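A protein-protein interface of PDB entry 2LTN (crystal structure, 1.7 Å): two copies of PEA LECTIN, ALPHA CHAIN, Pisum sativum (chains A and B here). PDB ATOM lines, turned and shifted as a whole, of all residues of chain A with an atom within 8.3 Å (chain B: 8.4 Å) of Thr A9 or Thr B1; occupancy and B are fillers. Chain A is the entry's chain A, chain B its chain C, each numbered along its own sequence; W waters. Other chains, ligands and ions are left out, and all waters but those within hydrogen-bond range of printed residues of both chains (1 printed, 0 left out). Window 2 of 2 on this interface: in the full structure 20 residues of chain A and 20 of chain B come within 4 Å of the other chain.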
ATOM      1  N   PHE A   6     -11.315  22.746 -34.871  1.00  0.00           N
ATOM      2  CA  PHE A   6     -10.698  21.576 -34.208  1.00  0.00           C
ATOM      3  C   PHE A   6      -9.779  22.140 -33.144  1.00  0.00           C
ATOM      4  O   PHE A   6      -9.364  23.295 -33.321  1.00  0.00           O
ATOM      5  CB  PHE A   6     -10.060  20.533 -35.079  1.00  0.00           C
ATOM      6  CG  PHE A   6      -8.841  21.015 -35.839  1.00  0.00           C
ATOM      7  CD1 PHE A   6      -8.983  21.456 -37.144  1.00  0.00           C
ATOM      8  CD2 PHE A   6      -7.618  21.014 -35.189  1.00  0.00           C
ATOM      9  CE1 PHE A   6      -7.826  21.930 -37.844  1.00  0.00           C
ATOM     10  CE2 PHE A   6      -6.457  21.479 -35.866  1.00  0.00           C
ATOM     11  CZ  PHE A   6      -6.613  21.869 -37.204  1.00  0.00           C
ATOM     12  N   LEU A   7      -9.571  21.369 -32.129  1.00  0.00           N
ATOM     13  CA  LEU A   7      -8.632  21.728 -31.041  1.00  0.00           C
ATOM     14  C   LEU A   7      -7.897  20.469 -30.705  1.00  0.00           C
ATOM     15  O   LEU A   7      -8.588  19.431 -30.425  1.00  0.00           O
ATOM     16  CB  LEU A   7      -9.394  22.326 -29.855  1.00  0.00           C
ATOM     17  CG  LEU A   7      -8.598  22.406 -28.561  1.00  0.00           C
ATOM     18  CD1 LEU A   7      -7.427  23.375 -28.703  1.00  0.00           C
ATOM     19  CD2 LEU A   7      -9.514  22.891 -27.440  1.00  0.00           C
ATOM     20  N   ILE A   8      -6.582  20.488 -30.596  1.00  0.00           N
ATOM     21  CA  ILE A   8      -5.803  19.352 -30.133  1.00  0.00           C
ATOM     22  C   ILE A   8      -4.829  19.898 -29.074  1.00  0.00           C
ATOM     23  O   ILE A   8      -3.944  20.689 -29.544  1.00  0.00           O
ATOM     24  CB  ILE A   8      -5.030  18.628 -31.253  1.00  0.00           C
ATOM     25  CG1 ILE A   8      -6.006  18.275 -32.417  1.00  0.00           C
ATOM     26  CG2 ILE A   8      -4.205  17.446 -30.636  1.00  0.00           C
ATOM     27  CD1 ILE A   8      -5.236  17.724 -33.672  1.00  0.00           C
ATOM     28  N   THR A   9      -5.065  19.534 -27.832  1.00  0.00           N
ATOM     29  CA  THR A   9      -4.100  20.113 -26.811  1.00  0.00           C
ATOM     30  C   THR A   9      -3.012  19.143 -26.507  1.00  0.00           C
ATOM     31  O   THR A   9      -2.076  19.584 -25.745  1.00  0.00           O
ATOM     32  CB  THR A   9      -4.835  20.655 -25.539  1.00  0.00           C
ATOM     33  OG1 THR A   9      -5.167  19.421 -24.832  1.00  0.00           O
ATOM     34  CG2 THR A   9      -6.056  21.534 -25.831  1.00  0.00           C
ATOM     35  N   LYS A  10      -3.058  17.934 -26.951  1.00  0.00           N
ATOM     36  CA  LYS A  10      -1.989  16.941 -26.736  1.00  0.00           C
ATOM     37  C   LYS A  10      -2.224  15.881 -27.804  1.00  0.00           C
ATOM     38  O   LYS A  10      -3.363  15.436 -28.058  1.00  0.00           O
ATOM     39  CB  LYS A  10      -1.729  16.446 -25.373  1.00  0.00           C
ATOM     40  CG  LYS A  10      -2.480  15.373 -24.677  1.00  0.00           C
ATOM     41  CD  LYS A  10      -2.708  14.079 -25.410  1.00  0.00           C
ATOM     42  CE  LYS A  10      -1.740  12.934 -25.167  1.00  0.00           C
ATOM     43  NZ  LYS A  10      -2.356  11.719 -25.836  1.00  0.00           N
ATOM     44  N   PHE A  11      -1.167  15.604 -28.526  1.00  0.00           N
ATOM     45  CA  PHE A  11      -1.197  14.694 -29.691  1.00  0.00           C
ATOM     46  C   PHE A  11      -1.130  13.254 -29.188  1.00  0.00           C
ATOM     47  O   PHE A  11      -0.534  13.064 -28.108  1.00  0.00           O
ATOM     48  CB  PHE A  11      -0.028  15.029 -30.639  1.00  0.00           C
ATOM     49  CG  PHE A  11      -0.253  16.357 -31.302  1.00  0.00           C
ATOM     50  CD1 PHE A  11      -1.054  16.442 -32.425  1.00  0.00           C
ATOM     51  CD2 PHE A  11       0.250  17.538 -30.736  1.00  0.00           C
ATOM     52  CE1 PHE A  11      -1.292  17.624 -33.087  1.00  0.00           C
ATOM     53  CE2 PHE A  11       0.034  18.765 -31.364  1.00  0.00           C
ATOM     54  CZ  PHE A  11      -0.736  18.814 -32.521  1.00  0.00           C
ATOM     55  N   SER A  12      -1.634  12.365 -29.967  1.00  0.00           N
ATOM     56  CA  SER A  12      -1.575  10.915 -29.643  1.00  0.00           C
ATOM     57  C   SER A  12      -0.691  10.281 -30.705  1.00  0.00           C
ATOM     58  O   SER A  12      -0.549  10.834 -31.813  1.00  0.00           O
ATOM     59  CB  SER A  12      -3.047  10.476 -29.679  1.00  0.00           C
ATOM     60  OG  SER A  12      -3.216   9.135 -30.112  1.00  0.00           O
ATOM     61  N   GLN A  15      -2.572   9.563 -34.486  1.00  0.00           N
ATOM     62  CA  GLN A  15      -3.460  10.773 -34.661  1.00  0.00           C
ATOM     63  C   GLN A  15      -4.050  10.687 -36.015  1.00  0.00           C
ATOM     64  O   GLN A  15      -3.508  11.208 -36.998  1.00  0.00           O
ATOM     65  CB  GLN A  15      -2.532  12.007 -34.425  1.00  0.00           C
ATOM     66  CG  GLN A  15      -3.306  13.314 -34.246  1.00  0.00           C
ATOM     67  CD  GLN A  15      -4.005  13.433 -32.948  1.00  0.00           C
ATOM     68  OE1 GLN A  15      -3.399  13.154 -31.910  1.00  0.00           O
ATOM     69  NE2 GLN A  15      -5.290  13.797 -32.929  1.00  0.00           N
ATOM     70  N   GLU A  29       3.298  13.144 -26.774  1.00  0.00           N
ATOM     71  CA  GLU A  29       2.120  14.030 -26.731  1.00  0.00           C
ATOM     72  C   GLU A  29       2.348  15.221 -27.701  1.00  0.00           C
ATOM     73  O   GLU A  29       1.504  16.158 -27.660  1.00  0.00           O
ATOM     74  CB  GLU A  29       1.953  14.691 -25.372  1.00  0.00           C
ATOM     75  CG  GLU A  29       1.965  13.912 -24.088  1.00  0.00           C
ATOM     76  CD  GLU A  29       1.991  14.673 -22.797  1.00  0.00           C
ATOM     77  OE1 GLU A  29       1.409  14.254 -21.787  1.00  0.00           O
ATOM     78  OE2 GLU A  29       2.648  15.746 -22.784  1.00  0.00           O
ATOM     79  N   LYS A  30       3.503  15.183 -28.369  1.00  0.00           N
ATOM     80  CA  LYS A  30       3.850  16.290 -29.288  1.00  0.00           C
ATOM     81  C   LYS A  30       3.887  15.849 -30.741  1.00  0.00           C
ATOM     82  O   LYS A  30       3.989  14.664 -31.044  1.00  0.00           O
ATOM     83  CB  LYS A  30       5.321  16.742 -29.029  1.00  0.00           C
ATOM     84  CG  LYS A  30       5.519  17.801 -28.008  1.00  0.00           C
ATOM     85  CD  LYS A  30       5.962  17.361 -26.626  1.00  0.00           C
ATOM     86  CE  LYS A  30       4.755  17.172 -25.696  1.00  0.00           C
ATOM     87  NZ  LYS A  30       3.676  16.493 -26.463  1.00  0.00           N
ATOM     88  N   THR A  68       1.226  26.257 -30.462  1.00  0.00           N
ATOM     89  CA  THR A  68       2.452  26.497 -29.644  1.00  0.00           C
ATOM     90  C   THR A  68       3.509  25.660 -30.307  1.00  0.00           C
ATOM     91  O   THR A  68       3.230  24.427 -30.559  1.00  0.00           O
ATOM     92  CB  THR A  68       2.236  26.094 -28.148  1.00  0.00           C
ATOM     93  OG1 THR A  68       1.171  26.935 -27.669  1.00  0.00           O
ATOM     94  CG2 THR A  68       3.539  26.226 -27.336  1.00  0.00           C
ATOM     95  N   THR B   1      -6.925  17.433 -24.467  1.00  0.00           N
ATOM     96  CA  THR B   1      -8.315  17.632 -24.957  1.00  0.00           C
ATOM     97  C   THR B   1      -8.336  17.615 -26.473  1.00  0.00           C
ATOM     98  O   THR B   1      -7.423  18.237 -27.062  1.00  0.00           O
ATOM     99  CB  THR B   1      -8.878  19.046 -24.484  1.00  0.00           C
ATOM    100  OG1 THR B   1      -8.729  19.015 -23.028  1.00  0.00           O
ATOM    101  CG2 THR B   1     -10.305  19.307 -24.936  1.00  0.00           C
ATOM    102  N   GLU B   2      -9.352  17.001 -27.065  1.00  0.00           N
ATOM    103  CA  GLU B   2      -9.480  16.974 -28.525  1.00  0.00           C
ATOM    104  C   GLU B   2     -10.909  17.234 -28.932  1.00  0.00           C
ATOM    105  O   GLU B   2     -11.800  16.497 -28.396  1.00  0.00           O
ATOM    106  CB  GLU B   2      -9.057  15.641 -29.102  1.00  0.00           C
ATOM    107  CG  GLU B   2      -7.576  15.308 -29.195  1.00  0.00           C
ATOM    108  CD  GLU B   2      -7.300  13.863 -29.534  1.00  0.00           C
ATOM    109  OE1 GLU B   2      -6.742  13.160 -28.688  1.00  0.00           O
ATOM    110  OE2 GLU B   2      -7.630  13.545 -30.657  1.00  0.00           O
ATOM    111  N   THR B   3     -11.130  18.282 -29.729  1.00  0.00           N
ATOM    112  CA  THR B   3     -12.518  18.573 -30.179  1.00  0.00           C
ATOM    113  C   THR B   3     -12.515  18.634 -31.675  1.00  0.00           C
ATOM    114  O   THR B   3     -11.515  18.955 -32.349  1.00  0.00           O
ATOM    115  CB  THR B   3     -13.117  19.840 -29.473  1.00  0.00           C
ATOM    116  OG1 THR B   3     -12.410  20.992 -30.125  1.00  0.00           O
ATOM    117  CG2 THR B   3     -12.814  19.906 -27.983  1.00  0.00           C
ATOM    118  N   THR B   4     -13.678  18.240 -32.250  1.00  0.00           N
ATOM    119  CA  THR B   4     -13.901  18.265 -33.719  1.00  0.00           C
ATOM    120  C   THR B   4     -15.252  18.910 -33.907  1.00  0.00           C
ATOM    121  O   THR B   4     -16.192  18.509 -33.179  1.00  0.00           O
ATOM    122  CB  THR B   4     -13.804  16.889 -34.435  1.00  0.00           C
ATOM    123  OG1 THR B   4     -12.482  16.339 -34.273  1.00  0.00           O
ATOM    124  CG2 THR B   4     -14.216  16.908 -35.907  1.00  0.00           C
ATOM    125  N   HIS B  51     -12.082  11.228 -33.104  1.00  0.00           N
ATOM    126  CA  HIS B  51     -11.518  10.479 -31.963  1.00  0.00           C
ATOM    127  C   HIS B  51     -12.600  10.404 -30.928  1.00  0.00           C
ATOM    128  O   HIS B  51     -12.972  11.353 -30.240  1.00  0.00           O
ATOM    129  CB  HIS B  51     -10.284  11.279 -31.431  1.00  0.00           C
ATOM    130  CG  HIS B  51      -9.408  10.333 -30.697  1.00  0.00           C
ATOM    131  ND1 HIS B  51      -8.245  10.741 -30.036  1.00  0.00           N
ATOM    132  CD2 HIS B  51      -9.536   9.027 -30.393  1.00  0.00           C
ATOM    133  CE1 HIS B  51      -7.694   9.690 -29.481  1.00  0.00           C
ATOM    134  NE2 HIS B  51      -8.426   8.638 -29.685  1.00  0.00           N
ATOM    135  N   ASN B  59     -11.040   7.446 -21.514  1.00  0.00           N
ATOM    136  CA  ASN B  59     -11.999   8.511 -21.756  1.00  0.00           C
ATOM    137  C   ASN B  59     -12.767   8.252 -23.067  1.00  0.00           C
ATOM    138  O   ASN B  59     -12.201   7.781 -24.040  1.00  0.00           O
ATOM    139  CB  ASN B  59     -11.397   9.913 -21.740  1.00  0.00           C
ATOM    140  CG  ASN B  59     -10.939  10.282 -20.352  1.00  0.00           C
ATOM    141  OD1 ASN B  59     -11.342   9.665 -19.347  1.00  0.00           O
ATOM    142  ND2 ASN B  59     -10.046  11.263 -20.237  1.00  0.00           N
HETATM  143  O   HOH W   1      -9.142  17.236 -32.854  1.00  0.00           O
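Among the printed residues, merely in contact across the chains: Leu A7 with Glu B2, Phe A6 with Thr B3, Ile A8 with Thr B1 and Leu A7 with Thr B1.
Water W1 bridges O of Thr B3 (3.0 Å) and O of Leu A7 (3.3 Å).
Of the printed residues of chain B, Phe A6 touches Thr B3 (3.3 Å).
Of the printed residues of chain B, Leu A7 touches Thr B1 (3.8 Å), Glu B2 (3.2 Å) and Thr B3 (2.9 Å).
Printed residues of chain B within 4 Å of Ile A8: Thr B1.
Thr A9 touches just one residue of chain B: Thr B1 (2.7 Å).
Printed residues of chain B within 4 Å of Gln A15: Glu B2.
Lys A30 touches none of the printed residues of chain B.
Thr B1 touches three residues of chain A.
Asn B59 touches none of the printed residues of chain A.
N of Thr B3 is in hydrogen-bond range of O of Leu A7, 2.9 Å away.
The backbone NH (N) of Thr B1 is in hydrogen-bond range of the side-chain hydroxyl (OG1) of Thr A9.
The side-chain carboxylate of Glu B2 lies within hydrogen-bond range of the side-chain amide nitrogen of Gln A15 (3.3 Å).
Of the 6 printed residues of chain B, 3 touch a printed residue of chain A.
Printed residues of chain B that touch a printed residue of chain A: Thr B1, Glu B2 and Thr B3.
Along chain B the printed residues that touch a printed residue of chain A span positions 1 to 3.
Among the printed residues, 7 pairs touch across the chains.
ND1 of His B51 lies within hydrogen-bond range of OE2 of Glu B2 (2.9 Å).
OE1 of Gln A15 is in hydrogen-bond range of N of Ser A12 (2.7 Å).
No position is printed for both chains.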
